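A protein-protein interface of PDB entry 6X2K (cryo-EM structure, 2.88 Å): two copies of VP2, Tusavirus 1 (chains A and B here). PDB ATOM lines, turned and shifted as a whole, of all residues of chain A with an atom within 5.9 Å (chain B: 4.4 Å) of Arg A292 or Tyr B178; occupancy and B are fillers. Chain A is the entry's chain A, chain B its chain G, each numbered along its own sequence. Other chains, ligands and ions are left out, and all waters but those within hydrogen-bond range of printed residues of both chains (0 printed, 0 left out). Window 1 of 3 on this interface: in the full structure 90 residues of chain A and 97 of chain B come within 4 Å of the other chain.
The backbone carbonyl oxygen (O) of Leu A254 is in hydrogen-bond range of the guanidinium group (NH2) of Arg B158.
OE1 of Gln B70 sits close to O of Pro A256.
The guanidinium group of Arg B158 is in salt-bridge range of the side-chain carboxylate of Glu A287 (3.2 Å).
The side-chain carboxylate (OE1) of Glu A287 is in hydrogen-bond range of the side-chain hydroxyl (OH) of Tyr B178, 3.4 Å away.
The side-chain sulfur (SG) of Cys B447 sits at hydrogen-bond distance from the backbone carbonyl oxygen (O) of Arg A292 (3.1 Å).
O of Pro A293 is in hydrogen-bond range of N of Cys B447 (3.4 Å).
NE of Arg B158 sits close to N of Pro A256, 3.5 Å away.
The guanidinium group (NH1) of Arg A292 is in hydrogen-bond range of the backbone carbonyl oxygen (O) of Arg A250 (3.4 Å).
The backbone carbonyl oxygen (O) of Leu A252 sits at hydrogen-bond distance from the guanidinium group (NH2) of Arg A292, at 2.6 Å.
The side-chain carboxylate (OE1) of Glu A287 is in salt-bridge range of the guanidinium group (NH1) of Arg A292 (3.3 Å).
Among the printed residues, pairs that only touch across the chains: Ser A251 with Tyr B178 (3.0 Å), Pro A255 with Gln B70 (3.2 Å), Val A290 with Arg B158 (3.4 Å), Gly A253 with Tyr B178 (3.4 Å), Pro A256 with His B68 (3.5 Å), Pro A255 with Tyr B178 (3.5 Å), Arg A292 with Tyr B178 (3.7 Å), Val A291 with Cys B447 (3.8 Å), Pro A255 with Arg B158 (3.8 Å), Pro A255 with Tyr B177 (3.8 Å), Trp A280 with Cys B447 (3.8 Å), Arg A250 with Tyr B178 (3.8 Å), Trp A246 with Tyr B178 (3.9 Å), Glu A287 with His B68 (3.9 Å), Leu A254 with Tyr B178 (3.9 Å) and Arg A250 with Trp B181 (3.95 Å).
Of the printed residues of chain B, Trp A246 touches Tyr B178.
Thr A249 touches none of the printed residues of chain B.
Of the printed residues of chain B, Arg A250 touches Tyr B178 and Trp B181.
Printed residues of chain B within 4 Å of Trp A280: Cys B447.
Of the printed residues of chain B, Glu A287 touches His B68, Arg B158 and Tyr B178.
Of chain B, only Tyr B178 and Cys B447 come within 4 Å of Arg A292.
Tyr B178 touches eight residues of chain A.
Printed residues of chain A within 4 Å of Cys B447: Trp A280, Val A291, Arg A292 and Pro A293.
The nearest residue of chain A that does not touch Tyr B178 is Leu A252 (4.1 Å).
The nearest printed residue of chain B that does not touch Pro A256 is Tyr B178 (4.3 Å).
Of the 9 printed residues of chain B, 7 touch a printed residue of chain A.
Printed residues of chain B that touch a printed residue of chain A: His B68, Gln B70, Arg B158, Tyr B177, Tyr B178, Trp B181 and Cys B447.
Of the 20 printed residues of chain A, 13 touch a printed residue of chain B.
Hydrophobic or aromatic side chains of chain A that line the printed part of chain B: Trp A246, Pro A255, Pro A256, Trp A280, Val A290 and Val A291.
Among the printed residues, 23 pairs touch across the chains.
Among the printed residues, Asp or Glu carboxylates within 4 Å of a Lys or Arg side-chain nitrogen of the other chain: Glu A287 with Arg B158.
No position is printed for both chains.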
ATOM      1  N   TRP A 246     -35.535  32.930 -21.317  1.00  0.00           N
ATOM      2  CA  TRP A 246     -35.423  31.495 -21.510  1.00  0.00           C
ATOM      3  C   TRP A 246     -34.024  30.978 -21.244  1.00  0.00           C
ATOM      4  O   TRP A 246     -33.843  29.767 -21.099  1.00  0.00           O
ATOM      5  CB  TRP A 246     -35.825  31.132 -22.932  1.00  0.00           C
ATOM      6  CG  TRP A 246     -35.029  31.847 -23.950  1.00  0.00           C
ATOM      7  CD1 TRP A 246     -35.313  33.046 -24.510  1.00  0.00           C
ATOM      8  CD2 TRP A 246     -33.797  31.419 -24.525  1.00  0.00           C
ATOM      9  NE1 TRP A 246     -34.341  33.392 -25.406  1.00  0.00           N
ATOM     10  CE2 TRP A 246     -33.397  32.404 -25.432  1.00  0.00           C
ATOM     11  CE3 TRP A 246     -32.994  30.292 -24.360  1.00  0.00           C
ATOM     12  CZ2 TRP A 246     -32.235  32.300 -26.168  1.00  0.00           C
ATOM     13  CZ3 TRP A 246     -31.848  30.192 -25.091  1.00  0.00           C
ATOM     14  CH2 TRP A 246     -31.476  31.186 -25.983  1.00  0.00           C
ATOM     15  N   GLN A 247     -33.037  31.858 -21.179  1.00  0.00           N
ATOM     16  CA  GLN A 247     -31.657  31.432 -21.085  1.00  0.00           C
ATOM     17  C   GLN A 247     -31.315  30.991 -19.675  1.00  0.00           C
ATOM     18  O   GLN A 247     -31.892  31.460 -18.696  1.00  0.00           O
ATOM     19  CB  GLN A 247     -30.724  32.554 -21.527  1.00  0.00           C
ATOM     20  CG  GLN A 247     -30.814  32.837 -22.996  1.00  0.00           C
ATOM     21  CD  GLN A 247     -29.901  33.934 -23.454  1.00  0.00           C
ATOM     22  OE1 GLN A 247     -29.564  34.824 -22.706  1.00  0.00           O
ATOM     23  NE2 GLN A 247     -29.478  33.859 -24.694  1.00  0.00           N
ATOM     24  N   THR A 249     -27.663  29.509 -17.246  1.00  0.00           N
ATOM     25  CA  THR A 249     -26.218  29.682 -17.206  1.00  0.00           C
ATOM     26  C   THR A 249     -25.572  29.095 -18.445  1.00  0.00           C
ATOM     27  O   THR A 249     -24.684  29.703 -19.040  1.00  0.00           O
ATOM     28  CB  THR A 249     -25.638  29.035 -15.955  1.00  0.00           C
ATOM     29  OG1 THR A 249     -26.147  29.697 -14.795  1.00  0.00           O
ATOM     30  CG2 THR A 249     -24.142  29.136 -15.961  1.00  0.00           C
ATOM     31  N   ARG A 250     -26.004  27.880 -18.788  1.00  0.00           N
ATOM     32  CA  ARG A 250     -25.469  27.085 -19.907  1.00  0.00           C
ATOM     33  C   ARG A 250     -25.759  27.540 -21.336  1.00  0.00           C
ATOM     34  O   ARG A 250     -25.149  27.059 -22.279  1.00  0.00           O
ATOM     35  CB  ARG A 250     -25.819  25.603 -19.733  1.00  0.00           C
ATOM     36  CG  ARG A 250     -24.888  24.893 -18.768  1.00  0.00           C
ATOM     37  CD  ARG A 250     -24.854  23.390 -18.975  1.00  0.00           C
ATOM     38  NE  ARG A 250     -24.779  23.032 -20.382  1.00  0.00           N
ATOM     39  CZ  ARG A 250     -24.666  21.791 -20.834  1.00  0.00           C
ATOM     40  NH1 ARG A 250     -24.598  20.774 -19.996  1.00  0.00           N
ATOM     41  NH2 ARG A 250     -24.613  21.569 -22.133  1.00  0.00           N
ATOM     42  N   SER A 251     -26.714  28.436 -21.490  1.00  0.00           N
ATOM     43  CA  SER A 251     -27.039  29.007 -22.786  1.00  0.00           C
ATOM     44  C   SER A 251     -26.432  30.386 -23.016  1.00  0.00           C
ATOM     45  O   SER A 251     -26.770  31.034 -24.005  1.00  0.00           O
ATOM     46  CB  SER A 251     -28.549  29.063 -22.962  1.00  0.00           C
ATOM     47  OG  SER A 251     -29.130  29.862 -21.959  1.00  0.00           O
ATOM     48  N   LEU A 252     -25.595  30.875 -22.112  1.00  0.00           N
ATOM     49  CA  LEU A 252     -25.020  32.213 -22.230  1.00  0.00           C
ATOM     50  C   LEU A 252     -23.674  32.125 -22.928  1.00  0.00           C
ATOM     51  O   LEU A 252     -22.730  31.560 -22.377  1.00  0.00           O
ATOM     52  CB  LEU A 252     -24.819  32.836 -20.858  1.00  0.00           C
ATOM     53  CG  LEU A 252     -25.960  33.102 -19.896  1.00  0.00           C
ATOM     54  CD1 LEU A 252     -25.355  33.564 -18.588  1.00  0.00           C
ATOM     55  CD2 LEU A 252     -26.909  34.133 -20.454  1.00  0.00           C
ATOM     56  N   GLY A 253     -23.575  32.653 -24.135  1.00  0.00           N
ATOM     57  CA  GLY A 253     -22.261  32.808 -24.713  1.00  0.00           C
ATOM     58  C   GLY A 253     -22.272  32.524 -26.193  1.00  0.00           C
ATOM     59  O   GLY A 253     -23.318  32.517 -26.834  1.00  0.00           O
ATOM     60  N   LEU A 254     -21.076  32.285 -26.721  1.00  0.00           N
ATOM     61  CA  LEU A 254     -20.917  31.776 -28.075  1.00  0.00           C
ATOM     62  C   LEU A 254     -20.851  30.259 -28.032  1.00  0.00           C
ATOM     63  O   LEU A 254     -20.009  29.711 -27.309  1.00  0.00           O
ATOM     64  CB  LEU A 254     -19.651  32.320 -28.695  1.00  0.00           C
ATOM     65  CG  LEU A 254     -19.298  31.843 -30.094  1.00  0.00           C
ATOM     66  CD1 LEU A 254     -20.355  32.277 -31.067  1.00  0.00           C
ATOM     67  CD2 LEU A 254     -17.962  32.389 -30.495  1.00  0.00           C
ATOM     68  N   PRO A 255     -21.720  29.545 -28.737  1.00  0.00           N
ATOM     69  CA  PRO A 255     -21.697  28.100 -28.675  1.00  0.00           C
ATOM     70  C   PRO A 255     -20.491  27.546 -29.404  1.00  0.00           C
ATOM     71  O   PRO A 255     -19.891  28.236 -30.237  1.00  0.00           O
ATOM     72  CB  PRO A 255     -23.013  27.698 -29.352  1.00  0.00           C
ATOM     73  CG  PRO A 255     -23.368  28.812 -30.171  1.00  0.00           C
ATOM     74  CD  PRO A 255     -22.880  30.032 -29.495  1.00  0.00           C
ATOM     75  N   PRO A 256     -20.106  26.307 -29.124  1.00  0.00           N
ATOM     76  CA  PRO A 256     -18.853  25.778 -29.664  1.00  0.00           C
ATOM     77  C   PRO A 256     -18.922  25.526 -31.161  1.00  0.00           C
ATOM     78  O   PRO A 256     -19.978  25.533 -31.795  1.00  0.00           O
ATOM     79  CB  PRO A 256     -18.680  24.471 -28.894  1.00  0.00           C
ATOM     80  CG  PRO A 256     -20.028  24.071 -28.564  1.00  0.00           C
ATOM     81  CD  PRO A 256     -20.759  25.329 -28.248  1.00  0.00           C
ATOM     82  N   TRP A 280     -13.089  26.409 -16.601  1.00  0.00           N
ATOM     83  CA  TRP A 280     -12.773  26.354 -15.182  1.00  0.00           C
ATOM     84  C   TRP A 280     -12.126  25.016 -14.863  1.00  0.00           C
ATOM     85  O   TRP A 280     -12.740  23.964 -15.059  1.00  0.00           O
ATOM     86  CB  TRP A 280     -14.027  26.542 -14.335  1.00  0.00           C
ATOM     87  CG  TRP A 280     -14.610  27.899 -14.398  1.00  0.00           C
ATOM     88  CD1 TRP A 280     -15.634  28.309 -15.181  1.00  0.00           C
ATOM     89  CD2 TRP A 280     -14.202  29.033 -13.642  1.00  0.00           C
ATOM     90  NE1 TRP A 280     -15.894  29.633 -14.965  1.00  0.00           N
ATOM     91  CE2 TRP A 280     -15.023  30.102 -14.020  1.00  0.00           C
ATOM     92  CE3 TRP A 280     -13.221  29.250 -12.679  1.00  0.00           C
ATOM     93  CZ2 TRP A 280     -14.893  31.364 -13.474  1.00  0.00           C
ATOM     94  CZ3 TRP A 280     -13.099  30.497 -12.136  1.00  0.00           C
ATOM     95  CH2 TRP A 280     -13.929  31.540 -12.530  1.00  0.00           C
ATOM     96  N   HIS A 286     -15.560  21.641 -22.210  1.00  0.00           N
ATOM     97  CA  HIS A 286     -16.880  21.056 -22.356  1.00  0.00           C
ATOM     98  C   HIS A 286     -17.903  22.108 -21.978  1.00  0.00           C
ATOM     99  O   HIS A 286     -17.574  23.121 -21.365  1.00  0.00           O
ATOM    100  CB  HIS A 286     -17.055  19.814 -21.477  1.00  0.00           C
ATOM    101  CG  HIS A 286     -16.145  18.682 -21.830  1.00  0.00           C
ATOM    102  ND1 HIS A 286     -16.343  17.887 -22.935  1.00  0.00           N
ATOM    103  CD2 HIS A 286     -15.029  18.215 -21.228  1.00  0.00           C
ATOM    104  CE1 HIS A 286     -15.392  16.975 -22.995  1.00  0.00           C
ATOM    105  NE2 HIS A 286     -14.580  17.154 -21.972  1.00  0.00           N
ATOM    106  N   GLU A 287     -19.160  21.860 -22.340  1.00  0.00           N
ATOM    107  CA  GLU A 287     -20.218  22.814 -22.037  1.00  0.00           C
ATOM    108  C   GLU A 287     -20.344  23.083 -20.553  1.00  0.00           C
ATOM    109  O   GLU A 287     -20.869  24.128 -20.163  1.00  0.00           O
ATOM    110  CB  GLU A 287     -21.546  22.311 -22.580  1.00  0.00           C
ATOM    111  CG  GLU A 287     -21.585  22.301 -24.072  1.00  0.00           C
ATOM    112  CD  GLU A 287     -21.392  23.673 -24.638  1.00  0.00           C
ATOM    113  OE1 GLU A 287     -22.046  24.613 -24.156  1.00  0.00           O
ATOM    114  OE2 GLU A 287     -20.550  23.823 -25.531  1.00  0.00           O
ATOM    115  N   THR A 288     -19.883  22.160 -19.721  1.00  0.00           N
ATOM    116  CA  THR A 288     -19.910  22.357 -18.284  1.00  0.00           C
ATOM    117  C   THR A 288     -18.759  23.223 -17.800  1.00  0.00           C
ATOM    118  O   THR A 288     -18.906  23.943 -16.813  1.00  0.00           O
ATOM    119  CB  THR A 288     -19.884  20.998 -17.598  1.00  0.00           C
ATOM    120  OG1 THR A 288     -18.716  20.290 -18.013  1.00  0.00           O
ATOM    121  CG2 THR A 288     -21.082  20.198 -18.006  1.00  0.00           C
ATOM    122  N   VAL A 290     -17.029  25.705 -19.506  1.00  0.00           N
ATOM    123  CA  VAL A 290     -16.718  26.962 -20.171  1.00  0.00           C
ATOM    124  C   VAL A 290     -16.895  28.133 -19.225  1.00  0.00           C
ATOM    125  O   VAL A 290     -17.892  28.224 -18.502  1.00  0.00           O
ATOM    126  CB  VAL A 290     -17.598  27.131 -21.412  1.00  0.00           C
ATOM    127  CG1 VAL A 290     -17.262  28.417 -22.107  1.00  0.00           C
ATOM    128  CG2 VAL A 290     -17.403  25.987 -22.334  1.00  0.00           C
ATOM    129  N   VAL A 291     -15.917  29.037 -19.221  1.00  0.00           N
ATOM    130  CA  VAL A 291     -16.076  30.292 -18.509  1.00  0.00           C
ATOM    131  C   VAL A 291     -17.194  31.080 -19.161  1.00  0.00           C
ATOM    132  O   VAL A 291     -17.271  31.182 -20.389  1.00  0.00           O
ATOM    133  CB  VAL A 291     -14.762  31.081 -18.507  1.00  0.00           C
ATOM    134  CG1 VAL A 291     -14.957  32.429 -17.872  1.00  0.00           C
ATOM    135  CG2 VAL A 291     -13.702  30.322 -17.768  1.00  0.00           C
ATOM    136  N   ARG A 292     -18.077  31.625 -18.346  1.00  0.00           N
ATOM    137  CA  ARG A 292     -19.252  32.346 -18.798  1.00  0.00           C
ATOM    138  C   ARG A 292     -19.306  33.664 -18.051  1.00  0.00           C
ATOM    139  O   ARG A 292     -18.594  33.840 -17.062  1.00  0.00           O
ATOM    140  CB  ARG A 292     -20.510  31.508 -18.549  1.00  0.00           C
ATOM    141  CG  ARG A 292     -20.472  30.234 -19.334  1.00  0.00           C
ATOM    142  CD  ARG A 292     -21.712  29.444 -19.176  1.00  0.00           C
ATOM    143  NE  ARG A 292     -21.646  28.183 -19.901  1.00  0.00           N
ATOM    144  CZ  ARG A 292     -21.905  28.048 -21.194  1.00  0.00           C
ATOM    145  NH1 ARG A 292     -21.829  26.859 -21.759  1.00  0.00           N
ATOM    146  NH2 ARG A 292     -22.233  29.101 -21.917  1.00  0.00           N
ATOM    147  N   PRO A 293     -20.099  34.630 -18.516  1.00  0.00           N
ATOM    148  CA  PRO A 293     -20.064  35.944 -17.863  1.00  0.00           C
ATOM    149  C   PRO A 293     -20.455  35.904 -16.400  1.00  0.00           C
ATOM    150  O   PRO A 293     -19.866  36.620 -15.585  1.00  0.00           O
ATOM    151  CB  PRO A 293     -21.049  36.761 -18.700  1.00  0.00           C
ATOM    152  CG  PRO A 293     -21.925  35.768 -19.320  1.00  0.00           C
ATOM    153  CD  PRO A 293     -21.044  34.626 -19.641  1.00  0.00           C
ATOM    154  N   CYS A 294     -21.436  35.087 -16.044  1.00  0.00           N
ATOM    155  CA  CYS A 294     -21.915  35.000 -14.676  1.00  0.00           C
ATOM    156  C   CYS A 294     -22.629  33.670 -14.521  1.00  0.00           C
ATOM    157  O   CYS A 294     -22.881  32.969 -15.501  1.00  0.00           O
ATOM    158  CB  CYS A 294     -22.829  36.175 -14.337  1.00  0.00           C
ATOM    159  SG  CYS A 294     -24.220  36.384 -15.441  1.00  0.00           S
ATOM    160  N   THR A 295     -22.917  33.306 -13.277  1.00  0.00           N
ATOM    161  CA  THR A 295     -23.802  32.187 -12.996  1.00  0.00           C
ATOM    162  C   THR A 295     -25.205  32.720 -12.769  1.00  0.00           C
ATOM    163  O   THR A 295     -25.388  33.730 -12.094  1.00  0.00           O
ATOM    164  CB  THR A 295     -23.367  31.409 -11.762  1.00  0.00           C
ATOM    165  OG1 THR A 295     -23.599  32.213 -10.610  1.00  0.00           O
ATOM    166  CG2 THR A 295     -21.901  31.107 -11.831  1.00  0.00           C
ATOM    167  N   HIS B  68     -26.282  20.217 -26.329  1.00  0.00           N
ATOM    168  CA  HIS B  68     -26.913  21.532 -26.416  1.00  0.00           C
ATOM    169  C   HIS B  68     -27.606  21.655 -27.768  1.00  0.00           C
ATOM    170  O   HIS B  68     -27.720  20.680 -28.514  1.00  0.00           O
ATOM    171  CB  HIS B  68     -25.890  22.650 -26.212  1.00  0.00           C
ATOM    172  CG  HIS B  68     -24.914  22.798 -27.334  1.00  0.00           C
ATOM    173  ND1 HIS B  68     -25.186  23.536 -28.462  1.00  0.00           N
ATOM    174  CD2 HIS B  68     -23.672  22.297 -27.508  1.00  0.00           C
ATOM    175  CE1 HIS B  68     -24.151  23.491 -29.278  1.00  0.00           C
ATOM    176  NE2 HIS B  68     -23.219  22.744 -28.721  1.00  0.00           N
ATOM    177  N   THR B  69     -28.085  22.859 -28.074  1.00  0.00           N
ATOM    178  CA  THR B  69     -28.733  23.165 -29.345  1.00  0.00           C
ATOM    179  C   THR B  69     -28.327  24.559 -29.782  1.00  0.00           C
ATOM    180  O   THR B  69     -28.404  25.500 -28.992  1.00  0.00           O
ATOM    181  CB  THR B  69     -30.255  23.091 -29.229  1.00  0.00           C
ATOM    182  OG1 THR B  69     -30.640  21.773 -28.831  1.00  0.00           O
ATOM    183  CG2 THR B  69     -30.900  23.404 -30.548  1.00  0.00           C
ATOM    184  N   GLN B  70     -27.916  24.703 -31.036  1.00  0.00           N
ATOM    185  CA  GLN B  70     -27.461  25.984 -31.544  1.00  0.00           C
ATOM    186  C   GLN B  70     -28.031  26.184 -32.935  1.00  0.00           C
ATOM    187  O   GLN B  70     -28.610  25.276 -33.526  1.00  0.00           O
ATOM    188  CB  GLN B  70     -25.938  26.069 -31.595  1.00  0.00           C
ATOM    189  CG  GLN B  70     -25.322  25.286 -32.722  1.00  0.00           C
ATOM    190  CD  GLN B  70     -23.821  25.317 -32.676  1.00  0.00           C
ATOM    191  OE1 GLN B  70     -23.228  25.412 -31.610  1.00  0.00           O
ATOM    192  NE2 GLN B  70     -23.195  25.289 -33.833  1.00  0.00           N
ATOM    193  N   ARG B 158     -13.409  30.664 -26.369  1.00  0.00           N
ATOM    194  CA  ARG B 158     -13.372  29.830 -27.563  1.00  0.00           C
ATOM    195  C   ARG B 158     -12.370  30.310 -28.601  1.00  0.00           C
ATOM    196  O   ARG B 158     -12.228  29.658 -29.635  1.00  0.00           O
ATOM    197  CB  ARG B 158     -14.758  29.660 -28.199  1.00  0.00           C
ATOM    198  CG  ARG B 158     -15.596  28.757 -27.342  1.00  0.00           C
ATOM    199  CD  ARG B 158     -16.904  28.390 -27.923  1.00  0.00           C
ATOM    200  NE  ARG B 158     -17.470  27.307 -27.131  1.00  0.00           N
ATOM    201  CZ  ARG B 158     -18.229  27.478 -26.065  1.00  0.00           C
ATOM    202  NH1 ARG B 158     -18.688  26.431 -25.406  1.00  0.00           N
ATOM    203  NH2 ARG B 158     -18.556  28.695 -25.677  1.00  0.00           N
ATOM    204  N   TYR B 177     -25.512  31.021 -32.507  1.00  0.00           N
ATOM    205  CA  TYR B 177     -26.029  31.355 -31.192  1.00  0.00           C
ATOM    206  C   TYR B 177     -26.894  30.213 -30.697  1.00  0.00           C
ATOM    207  O   TYR B 177     -27.283  29.328 -31.458  1.00  0.00           O
ATOM    208  CB  TYR B 177     -26.782  32.688 -31.214  1.00  0.00           C
ATOM    209  CG  TYR B 177     -27.968  32.766 -32.135  1.00  0.00           C
ATOM    210  CD1 TYR B 177     -29.239  32.482 -31.684  1.00  0.00           C
ATOM    211  CD2 TYR B 177     -27.821  33.147 -33.449  1.00  0.00           C
ATOM    212  CE1 TYR B 177     -30.316  32.571 -32.514  1.00  0.00           C
ATOM    213  CE2 TYR B 177     -28.892  33.227 -34.284  1.00  0.00           C
ATOM    214  CZ  TYR B 177     -30.136  32.940 -33.814  1.00  0.00           C
ATOM    215  OH  TYR B 177     -31.218  33.025 -34.654  1.00  0.00           O
ATOM    216  N   TYR B 178     -27.157  30.216 -29.399  1.00  0.00           N
ATOM    217  CA  TYR B 178     -27.925  29.145 -28.796  1.00  0.00           C
ATOM    218  C   TYR B 178     -29.404  29.269 -29.133  1.00  0.00           C
ATOM    219  O   TYR B 178     -29.919  30.349 -29.421  1.00  0.00           O
ATOM    220  CB  TYR B 178     -27.766  29.144 -27.283  1.00  0.00           C
ATOM    221  CG  TYR B 178     -26.407  28.758 -26.775  1.00  0.00           C
ATOM    222  CD1 TYR B 178     -26.057  27.436 -26.630  1.00  0.00           C
ATOM    223  CD2 TYR B 178     -25.493  29.714 -26.394  1.00  0.00           C
ATOM    224  CE1 TYR B 178     -24.833  27.082 -26.152  1.00  0.00           C
ATOM    225  CE2 TYR B 178     -24.272  29.364 -25.909  1.00  0.00           C
ATOM    226  CZ  TYR B 178     -23.948  28.049 -25.791  1.00  0.00           C
ATOM    227  OH  TYR B 178     -22.720  27.698 -25.308  1.00  0.00           O
ATOM    228  N   PHE B 179     -30.091  28.138 -29.073  1.00  0.00           N
ATOM    229  CA  PHE B 179     -31.523  28.061 -29.284  1.00  0.00           C
ATOM    230  C   PHE B 179     -32.083  27.175 -28.185  1.00  0.00           C
ATOM    231  O   PHE B 179     -31.468  26.174 -27.828  1.00  0.00           O
ATOM    232  CB  PHE B 179     -31.838  27.498 -30.661  1.00  0.00           C
ATOM    233  CG  PHE B 179     -33.287  27.510 -31.006  1.00  0.00           C
ATOM    234  CD1 PHE B 179     -33.886  28.664 -31.459  1.00  0.00           C
ATOM    235  CD2 PHE B 179     -34.046  26.367 -30.914  1.00  0.00           C
ATOM    236  CE1 PHE B 179     -35.208  28.677 -31.790  1.00  0.00           C
ATOM    237  CE2 PHE B 179     -35.367  26.383 -31.244  1.00  0.00           C
ATOM    238  CZ  PHE B 179     -35.948  27.541 -31.682  1.00  0.00           C
ATOM    239  N   TRP B 181     -33.478  24.787 -25.367  1.00  0.00           N
ATOM    240  CA  TRP B 181     -33.613  23.339 -25.263  1.00  0.00           C
ATOM    241  C   TRP B 181     -33.807  22.959 -23.803  1.00  0.00           C
ATOM    242  O   TRP B 181     -33.550  23.753 -22.899  1.00  0.00           O
ATOM    243  CB  TRP B 181     -32.398  22.593 -25.826  1.00  0.00           C
ATOM    244  CG  TRP B 181     -31.162  22.632 -24.979  1.00  0.00           C
ATOM    245  CD1 TRP B 181     -30.743  21.672 -24.109  1.00  0.00           C
ATOM    246  CD2 TRP B 181     -30.185  23.671 -24.918  1.00  0.00           C
ATOM    247  NE1 TRP B 181     -29.572  22.047 -23.515  1.00  0.00           N
ATOM    248  CE2 TRP B 181     -29.208  23.274 -23.993  1.00  0.00           C
ATOM    249  CE3 TRP B 181     -30.044  24.899 -25.551  1.00  0.00           C
ATOM    250  CZ2 TRP B 181     -28.112  24.060 -23.693  1.00  0.00           C
ATOM    251  CZ3 TRP B 181     -28.961  25.674 -25.252  1.00  0.00           C
ATOM    252  CH2 TRP B 181     -28.005  25.255 -24.333  1.00  0.00           C
ATOM    253  N   CYS B 447     -16.636  36.963 -14.754  1.00  0.00           N
ATOM    254  CA  CYS B 447     -15.663  35.897 -14.593  1.00  0.00           C
ATOM    255  C   CYS B 447     -14.363  36.155 -15.331  1.00  0.00           C
ATOM    256  O   CYS B 447     -13.337  35.596 -14.944  1.00  0.00           O
ATOM    257  CB  CYS B 447     -16.265  34.578 -15.067  1.00  0.00           C
ATOM    258  SG  CYS B 447     -17.674  34.011 -14.114  1.00  0.00           S
